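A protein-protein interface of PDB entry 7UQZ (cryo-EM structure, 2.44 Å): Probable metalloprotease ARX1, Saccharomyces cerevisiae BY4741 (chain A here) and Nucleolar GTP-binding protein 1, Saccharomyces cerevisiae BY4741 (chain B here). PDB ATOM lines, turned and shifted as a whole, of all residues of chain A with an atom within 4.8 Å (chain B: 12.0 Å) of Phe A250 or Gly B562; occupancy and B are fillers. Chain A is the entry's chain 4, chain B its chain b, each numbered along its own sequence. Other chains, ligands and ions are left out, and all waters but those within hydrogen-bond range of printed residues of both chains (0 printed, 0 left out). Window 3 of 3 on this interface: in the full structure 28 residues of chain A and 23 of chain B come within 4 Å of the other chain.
The backbone carbonyl oxygen (O) of Val A387 is in hydrogen-bond range of the side-chain amide nitrogen (NE2) of Gln A254, 3.1 Å away. The backbone NH of Arg B561 sits at hydrogen-bond distance from the side-chain carboxylate of Asp B564, 3.1 Å away. The backbone NH (N) of Phe A250 sits at hydrogen-bond distance from the backbone carbonyl oxygen (O) of Gly A149, 2.8 Å away. The backbone NH of Asp A148 lies within hydrogen-bond range of the backbone carbonyl oxygen of Glu A86 (2.8 Å). The backbone carbonyl oxygen (O) of Val B566 sits close to the side-chain amide nitrogen (NE2) of Gln B570, 3.3 Å away.
Among the printed residues, pairs that only touch across the chains: Phe A250 with Val B566 (3.4 Å), Glu A86 with Arg B561 (3.4 Å), Val A387 with Gly B562 (3.5 Å), Val A387 with Ser B563 (3.6 Å), Phe A250 with Gly B562 (3.7 Å), Leu A251 with Val B566 (3.97 Å), Glu A86 with Gly B562 (3.97 Å) and Val A387 with Val B566 (3.999 Å).
Phe A250 touches two residues of chain B. Glu A86 touches just these residues of chain B: Arg B561 (3.4 Å) and Gly B562 (3.97 Å). No residue of chain B comes within 4 Å of Asp A148. No residue of chain B comes within 4 Å of Gly A149. No residue of chain B comes within 4 Å of Arg A249. No residue of chain B comes within 4 Å of Ala A252. Printed residues of chain A within 4 Å of Arg B561: Glu A86 (3.4 Å). Of the printed residues of chain A, Val B566 touches Phe A250 (3.4 Å), Leu A251 (3.97 Å) and Val A387 (3.999 Å). Printed residues of chain A within 4 Å of Ser B563: Val A387. Of the printed residues of chain B, Val A387 touches Gly B562, Ser B563 and Val B566. The nearest residue of chain B that does not touch Phe A250 is Val B565 (4.2 Å).
Hydrophobic or aromatic side chains of chain A within 4 Å of the printed part of chain B: Phe A250, Leu A251 and Val A387. Of the 14 printed residues of chain B, 4 touch a printed residue of chain A. Printed residues of chain B that touch a printed residue of chain A: Arg B561, Gly B562, Ser B563 and Val B566. Hydrophobic or aromatic side chains of chain B that line the printed part of chain A: Val B566. Among the printed residues, 8 pairs touch across the chains. Among the printed residues, no Asp or Glu carboxylate lies within 4 Å of a Lys or Arg side-chain nitrogen of the other chain.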
ATOM      1  N   GLU A  86       0.752 -15.387  32.886  1.00  0.00           N
ATOM      2  CA  GLU A  86       0.073 -14.500  31.951  1.00  0.00           C
ATOM      3  C   GLU A  86      -1.195 -15.158  31.431  1.00  0.00           C
ATOM      4  O   GLU A  86      -1.176 -16.325  31.028  1.00  0.00           O
ATOM      5  CB  GLU A  86       0.992 -14.129  30.779  1.00  0.00           C
ATOM      6  CG  GLU A  86       2.277 -13.436  31.199  1.00  0.00           C
ATOM      7  CD  GLU A  86       3.188 -13.130  30.029  1.00  0.00           C
ATOM      8  OE1 GLU A  86       2.748 -13.285  28.873  1.00  0.00           O
ATOM      9  OE2 GLU A  86       4.348 -12.734  30.270  1.00  0.00           O
ATOM     10  N   HIS A 146      -6.567 -17.031  25.960  1.00  0.00           N
ATOM     11  CA  HIS A 146      -5.286 -17.693  26.164  1.00  0.00           C
ATOM     12  C   HIS A 146      -4.986 -17.818  27.651  1.00  0.00           C
ATOM     13  O   HIS A 146      -5.322 -16.930  28.442  1.00  0.00           O
ATOM     14  CB  HIS A 146      -4.148 -16.943  25.453  1.00  0.00           C
ATOM     15  CG  HIS A 146      -3.578 -15.806  26.241  1.00  0.00           C
ATOM     16  ND1 HIS A 146      -2.473 -15.945  27.053  1.00  0.00           N
ATOM     17  CD2 HIS A 146      -3.957 -14.510  26.341  1.00  0.00           C
ATOM     18  CE1 HIS A 146      -2.196 -14.784  27.619  1.00  0.00           C
ATOM     19  NE2 HIS A 146      -3.082 -13.897  27.204  1.00  0.00           N
ATOM     20  N   ASP A 148      -1.522 -18.898  29.860  1.00  0.00           N
ATOM     21  CA  ASP A 148      -0.084 -19.187  29.812  1.00  0.00           C
ATOM     22  C   ASP A 148       0.428 -19.291  28.377  1.00  0.00           C
ATOM     23  O   ASP A 148       1.356 -20.050  28.088  1.00  0.00           O
ATOM     24  CB  ASP A 148       0.259 -20.456  30.600  1.00  0.00           C
ATOM     25  CG  ASP A 148       1.708 -20.497  31.041  1.00  0.00           C
ATOM     26  OD1 ASP A 148       2.437 -19.518  30.779  1.00  0.00           O
ATOM     27  OD2 ASP A 148       2.118 -21.510  31.646  1.00  0.00           O
ATOM     28  N   GLY A 149      -0.170 -18.528  27.466  1.00  0.00           N
ATOM     29  CA  GLY A 149       0.207 -18.563  26.072  1.00  0.00           C
ATOM     30  C   GLY A 149      -0.467 -19.635  25.246  1.00  0.00           C
ATOM     31  O   GLY A 149      -0.277 -19.658  24.023  1.00  0.00           O
ATOM     32  N   ARG A 248       1.256 -23.184  18.603  1.00  0.00           N
ATOM     33  CA  ARG A 248       2.139 -23.450  19.731  1.00  0.00           C
ATOM     34  C   ARG A 248       1.916 -22.388  20.807  1.00  0.00           C
ATOM     35  O   ARG A 248       1.012 -21.554  20.709  1.00  0.00           O
ATOM     36  CB  ARG A 248       3.601 -23.502  19.280  1.00  0.00           C
ATOM     37  CG  ARG A 248       3.963 -24.767  18.520  1.00  0.00           C
ATOM     38  CD  ARG A 248       5.469 -24.982  18.459  1.00  0.00           C
ATOM     39  NE  ARG A 248       6.126 -24.126  17.479  1.00  0.00           N
ATOM     40  CZ  ARG A 248       6.811 -23.029  17.776  1.00  0.00           C
ATOM     41  NH1 ARG A 248       6.941 -22.612  19.024  1.00  0.00           N
ATOM     42  NH2 ARG A 248       7.386 -22.337  16.796  1.00  0.00           N
ATOM     43  N   ARG A 249       2.748 -22.432  21.845  1.00  0.00           N
ATOM     44  CA  ARG A 249       2.626 -21.497  22.956  1.00  0.00           C
ATOM     45  C   ARG A 249       3.055 -20.101  22.518  1.00  0.00           C
ATOM     46  O   ARG A 249       4.144 -19.922  21.963  1.00  0.00           O
ATOM     47  CB  ARG A 249       3.474 -21.973  24.134  1.00  0.00           C
ATOM     48  CG  ARG A 249       3.348 -21.140  25.398  1.00  0.00           C
ATOM     49  CD  ARG A 249       4.032 -21.840  26.561  1.00  0.00           C
ATOM     50  NE  ARG A 249       4.122 -21.001  27.750  1.00  0.00           N
ATOM     51  CZ  ARG A 249       5.213 -20.346  28.120  1.00  0.00           C
ATOM     52  NH1 ARG A 249       6.330 -20.410  27.414  1.00  0.00           N
ATOM     53  NH2 ARG A 249       5.186 -19.612  29.229  1.00  0.00           N
ATOM     54  N   PHE A 250       2.174 -19.120  22.748  1.00  0.00           N
ATOM     55  CA  PHE A 250       2.356 -17.715  22.381  1.00  0.00           C
ATOM     56  C   PHE A 250       2.476 -17.503  20.874  1.00  0.00           C
ATOM     57  O   PHE A 250       2.758 -16.388  20.425  1.00  0.00           O
ATOM     58  CB  PHE A 250       3.577 -17.110  23.083  1.00  0.00           C
ATOM     59  CG  PHE A 250       3.376 -16.860  24.548  1.00  0.00           C
ATOM     60  CD1 PHE A 250       2.504 -15.875  24.981  1.00  0.00           C
ATOM     61  CD2 PHE A 250       4.075 -17.590  25.491  1.00  0.00           C
ATOM     62  CE1 PHE A 250       2.322 -15.635  26.328  1.00  0.00           C
ATOM     63  CE2 PHE A 250       3.898 -17.355  26.840  1.00  0.00           C
ATOM     64  CZ  PHE A 250       3.021 -16.376  27.260  1.00  0.00           C
ATOM     65  N   LEU A 251       2.261 -18.553  20.085  1.00  0.00           N
ATOM     66  CA  LEU A 251       2.297 -18.482  18.627  1.00  0.00           C
ATOM     67  C   LEU A 251       1.010 -19.115  18.111  1.00  0.00           C
ATOM     68  O   LEU A 251       0.976 -20.302  17.781  1.00  0.00           O
ATOM     69  CB  LEU A 251       3.534 -19.182  18.068  1.00  0.00           C
ATOM     70  CG  LEU A 251       4.890 -18.605  18.475  1.00  0.00           C
ATOM     71  CD1 LEU A 251       6.018 -19.470  17.946  1.00  0.00           C
ATOM     72  CD2 LEU A 251       5.034 -17.177  17.979  1.00  0.00           C
ATOM     73  N   ALA A 252      -0.052 -18.314  18.041  1.00  0.00           N
ATOM     74  CA  ALA A 252      -1.353 -18.790  17.589  1.00  0.00           C
ATOM     75  C   ALA A 252      -1.811 -18.114  16.306  1.00  0.00           C
ATOM     76  O   ALA A 252      -2.934 -18.363  15.854  1.00  0.00           O
ATOM     77  CB  ALA A 252      -2.404 -18.587  18.683  1.00  0.00           C
ATOM     78  N   GLN A 254      -2.376 -14.885  16.149  1.00  0.00           N
ATOM     79  CA  GLN A 254      -3.310 -13.833  16.537  1.00  0.00           C
ATOM     80  C   GLN A 254      -3.098 -12.571  15.712  1.00  0.00           C
ATOM     81  O   GLN A 254      -4.034 -11.782  15.536  1.00  0.00           O
ATOM     82  CB  GLN A 254      -3.180 -13.526  18.031  1.00  0.00           C
ATOM     83  CG  GLN A 254      -1.796 -13.090  18.484  1.00  0.00           C
ATOM     84  CD  GLN A 254      -0.948 -14.246  18.975  1.00  0.00           C
ATOM     85  OE1 GLN A 254      -1.236 -15.407  18.692  1.00  0.00           O
ATOM     86  NE2 GLN A 254       0.099 -13.932  19.727  1.00  0.00           N
ATOM     87  N   VAL A 387       1.544 -10.259  24.266  1.00  0.00           N
ATOM     88  CA  VAL A 387       1.783 -10.269  22.825  1.00  0.00           C
ATOM     89  C   VAL A 387       0.499 -10.564  22.064  1.00  0.00           C
ATOM     90  O   VAL A 387       0.533 -11.103  20.952  1.00  0.00           O
ATOM     91  CB  VAL A 387       2.877 -11.286  22.453  1.00  0.00           C
ATOM     92  CG1 VAL A 387       4.227 -10.795  22.920  1.00  0.00           C
ATOM     93  CG2 VAL A 387       2.565 -12.646  23.053  1.00  0.00           C
ATOM     94  N   TYR A 388      -0.636 -10.214  22.647  1.00  0.00           N
ATOM     95  CA  TYR A 388      -1.902 -10.398  21.963  1.00  0.00           C
ATOM     96  C   TYR A 388      -2.552  -9.045  21.684  1.00  0.00           C
ATOM     97  O   TYR A 388      -2.272  -8.067  22.384  1.00  0.00           O
ATOM     98  CB  TYR A 388      -2.849 -11.272  22.795  1.00  0.00           C
ATOM     99  CG  TYR A 388      -2.368 -12.698  22.943  1.00  0.00           C
ATOM    100  CD1 TYR A 388      -2.695 -13.664  22.000  1.00  0.00           C
ATOM    101  CD2 TYR A 388      -1.576 -13.077  24.019  1.00  0.00           C
ATOM    102  CE1 TYR A 388      -2.254 -14.966  22.127  1.00  0.00           C
ATOM    103  CE2 TYR A 388      -1.130 -14.377  24.155  1.00  0.00           C
ATOM    104  CZ  TYR A 388      -1.473 -15.317  23.208  1.00  0.00           C
ATOM    105  OH  TYR A 388      -1.031 -16.612  23.340  1.00  0.00           O
ATOM    106  N   TYR B 558      16.224 -15.046  35.535  1.00  0.00           N
ATOM    107  CA  TYR B 558      15.648 -14.575  34.282  1.00  0.00           C
ATOM    108  C   TYR B 558      14.587 -15.564  33.814  1.00  0.00           C
ATOM    109  O   TYR B 558      14.898 -16.725  33.527  1.00  0.00           O
ATOM    110  CB  TYR B 558      16.727 -14.399  33.214  1.00  0.00           C
ATOM    111  CG  TYR B 558      16.174 -14.304  31.810  1.00  0.00           C
ATOM    112  CD1 TYR B 558      15.471 -13.180  31.392  1.00  0.00           C
ATOM    113  CD2 TYR B 558      16.354 -15.340  30.901  1.00  0.00           C
ATOM    114  CE1 TYR B 558      14.962 -13.091  30.108  1.00  0.00           C
ATOM    115  CE2 TYR B 558      15.849 -15.259  29.616  1.00  0.00           C
ATOM    116  CZ  TYR B 558      15.155 -14.133  29.225  1.00  0.00           C
ATOM    117  OH  TYR B 558      14.652 -14.052  27.946  1.00  0.00           O
ATOM    118  N   VAL B 559      13.343 -15.099  33.726  1.00  0.00           N
ATOM    119  CA  VAL B 559      12.216 -15.916  33.289  1.00  0.00           C
ATOM    120  C   VAL B 559      11.696 -15.349  31.977  1.00  0.00           C
ATOM    121  O   VAL B 559      11.368 -14.160  31.894  1.00  0.00           O
ATOM    122  CB  VAL B 559      11.102 -15.959  34.349  1.00  0.00           C
ATOM    123  CG1 VAL B 559       9.962 -16.855  33.884  1.00  0.00           C
ATOM    124  CG2 VAL B 559      11.654 -16.440  35.681  1.00  0.00           C
ATOM    125  N   GLU B 560      11.622 -16.198  30.956  1.00  0.00           N
ATOM    126  CA  GLU B 560      11.144 -15.764  29.654  1.00  0.00           C
ATOM    127  C   GLU B 560       9.647 -15.475  29.693  1.00  0.00           C
ATOM    128  O   GLU B 560       8.901 -16.009  30.518  1.00  0.00           O
ATOM    129  CB  GLU B 560      11.442 -16.819  28.589  1.00  0.00           C
ATOM    130  CG  GLU B 560      12.919 -17.006  28.295  1.00  0.00           C
ATOM    131  CD  GLU B 560      13.163 -17.939  27.125  1.00  0.00           C
ATOM    132  OE1 GLU B 560      12.194 -18.575  26.658  1.00  0.00           O
ATOM    133  OE2 GLU B 560      14.321 -18.033  26.668  1.00  0.00           O
ATOM    134  N   ARG B 561       9.215 -14.607  28.783  1.00  0.00           N
ATOM    135  CA  ARG B 561       7.818 -14.220  28.653  1.00  0.00           C
ATOM    136  C   ARG B 561       7.402 -14.336  27.192  1.00  0.00           C
ATOM    137  O   ARG B 561       8.194 -14.722  26.323  1.00  0.00           O
ATOM    138  CB  ARG B 561       7.583 -12.798  29.176  1.00  0.00           C
ATOM    139  CG  ARG B 561       7.736 -12.646  30.681  1.00  0.00           C
ATOM    140  CD  ARG B 561       7.266 -11.276  31.147  1.00  0.00           C
ATOM    141  NE  ARG B 561       8.127 -10.203  30.665  1.00  0.00           N
ATOM    142  CZ  ARG B 561       9.086  -9.634  31.381  1.00  0.00           C
ATOM    143  NH1 ARG B 561       9.329 -10.002  32.628  1.00  0.00           N
ATOM    144  NH2 ARG B 561       9.817  -8.667  30.835  1.00  0.00           N
ATOM    145  N   GLY B 562       6.138 -13.998  26.928  1.00  0.00           N
ATOM    146  CA  GLY B 562       5.641 -14.020  25.564  1.00  0.00           C
ATOM    147  C   GLY B 562       6.369 -13.058  24.650  1.00  0.00           C
ATOM    148  O   GLY B 562       6.568 -13.352  23.468  1.00  0.00           O
ATOM    149  N   SER B 563       6.770 -11.897  25.175  1.00  0.00           N
ATOM    150  CA  SER B 563       7.554 -10.958  24.378  1.00  0.00           C
ATOM    151  C   SER B 563       8.897 -11.559  23.988  1.00  0.00           C
ATOM    152  O   SER B 563       9.347 -11.401  22.848  1.00  0.00           O
ATOM    153  CB  SER B 563       7.742  -9.648  25.143  1.00  0.00           C
ATOM    154  OG  SER B 563       8.320  -9.874  26.416  1.00  0.00           O
ATOM    155  N   ASP B 564       9.545 -12.266  24.916  1.00  0.00           N
ATOM    156  CA  ASP B 564      10.796 -12.942  24.594  1.00  0.00           C
ATOM    157  C   ASP B 564      10.584 -14.073  23.597  1.00  0.00           C
ATOM    158  O   ASP B 564      11.455 -14.330  22.760  1.00  0.00           O
ATOM    159  CB  ASP B 564      11.449 -13.481  25.866  1.00  0.00           C
ATOM    160  CG  ASP B 564      11.683 -12.404  26.903  1.00  0.00           C
ATOM    161  OD1 ASP B 564      11.971 -11.253  26.514  1.00  0.00           O
ATOM    162  OD2 ASP B 564      11.580 -12.711  28.108  1.00  0.00           O
ATOM    163  N   VAL B 565       9.448 -14.768  23.678  1.00  0.00           N
ATOM    164  CA  VAL B 565       9.195 -15.871  22.756  1.00  0.00           C
ATOM    165  C   VAL B 565       8.942 -15.353  21.344  1.00  0.00           C
ATOM    166  O   VAL B 565       9.485 -15.884  20.367  1.00  0.00           O
ATOM    167  CB  VAL B 565       8.024 -16.736  23.263  1.00  0.00           C
ATOM    168  CG1 VAL B 565       7.617 -17.757  22.207  1.00  0.00           C
ATOM    169  CG2 VAL B 565       8.408 -17.435  24.552  1.00  0.00           C
ATOM    170  N   VAL B 566       8.133 -14.306  21.206  1.00  0.00           N
ATOM    171  CA  VAL B 566       7.692 -13.860  19.886  1.00  0.00           C
ATOM    172  C   VAL B 566       8.688 -12.892  19.255  1.00  0.00           C
ATOM    173  O   VAL B 566       9.039 -13.030  18.081  1.00  0.00           O
ATOM    174  CB  VAL B 566       6.281 -13.239  19.977  1.00  0.00           C
ATOM    175  CG1 VAL B 566       5.793 -12.833  18.598  1.00  0.00           C
ATOM    176  CG2 VAL B 566       5.312 -14.221  20.610  1.00  0.00           C
ATOM    177  N   PHE B 567       9.156 -11.895  20.009  1.00  0.00           N
ATOM    178  CA  PHE B 567      10.042 -10.862  19.485  1.00  0.00           C
ATOM    179  C   PHE B 567      11.464 -10.983  20.020  1.00  0.00           C
ATOM    180  O   PHE B 567      12.184  -9.981  20.083  1.00  0.00           O
ATOM    181  CB  PHE B 567       9.485  -9.473  19.803  1.00  0.00           C
ATOM    182  CG  PHE B 567       8.118  -9.223  19.243  1.00  0.00           C
ATOM    183  CD1 PHE B 567       7.958  -8.791  17.936  1.00  0.00           C
ATOM    184  CD2 PHE B 567       6.988  -9.412  20.024  1.00  0.00           C
ATOM    185  CE1 PHE B 567       6.698  -8.559  17.418  1.00  0.00           C
ATOM    186  CE2 PHE B 567       5.727  -9.182  19.513  1.00  0.00           C
ATOM    187  CZ  PHE B 567       5.582  -8.753  18.209  1.00  0.00           C
ATOM    188  N   GLY B 568      11.881 -12.185  20.423  1.00  0.00           N
ATOM    189  CA  GLY B 568      13.215 -12.345  20.981  1.00  0.00           C
ATOM    190  C   GLY B 568      14.319 -12.109  19.968  1.00  0.00           C
ATOM    191  O   GLY B 568      15.321 -11.454  20.271  1.00  0.00           O
ATOM    192  N   ASP B 569      14.157 -12.638  18.756  1.00  0.00           N
ATOM    193  CA  ASP B 569      15.141 -12.478  17.698  1.00  0.00           C
ATOM    194  C   ASP B 569      14.662 -11.598  16.553  1.00  0.00           C
ATOM    195  O   ASP B 569      15.480 -11.200  15.717  1.00  0.00           O
ATOM    196  CB  ASP B 569      15.548 -13.849  17.139  1.00  0.00           C
ATOM    197  CG  ASP B 569      14.354 -14.684  16.728  1.00  0.00           C
ATOM    198  OD1 ASP B 569      13.347 -14.679  17.466  1.00  0.00           O
ATOM    199  OD2 ASP B 569      14.419 -15.342  15.666  1.00  0.00           O
ATOM    200  N   GLN B 570      13.371 -11.289  16.490  1.00  0.00           N
ATOM    201  CA  GLN B 570      12.838 -10.468  15.418  1.00  0.00           C
ATOM    202  C   GLN B 570      13.203  -9.002  15.629  1.00  0.00           C
ATOM    203  O   GLN B 570      13.666  -8.591  16.697  1.00  0.00           O
ATOM    204  CB  GLN B 570      11.321 -10.631  15.324  1.00  0.00           C
ATOM    205  CG  GLN B 570      10.872 -12.058  15.071  1.00  0.00           C
ATOM    206  CD  GLN B 570       9.367 -12.180  14.950  1.00  0.00           C
ATOM    207  OE1 GLN B 570       8.646 -11.184  14.992  1.00  0.00           O
ATOM    208  NE2 GLN B 570       8.884 -13.409  14.795  1.00  0.00           N
ATOM    209  N   LEU B 573       9.440  -4.733  12.203  1.00  0.00           N
ATOM    210  CA  LEU B 573       7.978  -4.797  12.151  1.00  0.00           C
ATOM    211  C   LEU B 573       7.360  -3.513  11.611  1.00  0.00           C
ATOM    212  O   LEU B 573       6.129  -3.392  11.591  1.00  0.00           O
ATOM    213  CB  LEU B 573       7.339  -5.133  13.507  1.00  0.00           C
ATOM    214  CG  LEU B 573       6.098  -6.027  13.444  1.00  0.00           C
ATOM    215  CD1 LEU B 573       6.476  -7.403  12.916  1.00  0.00           C
ATOM    216  CD2 LEU B 573       5.412  -6.127  14.798  1.00  0.00           C
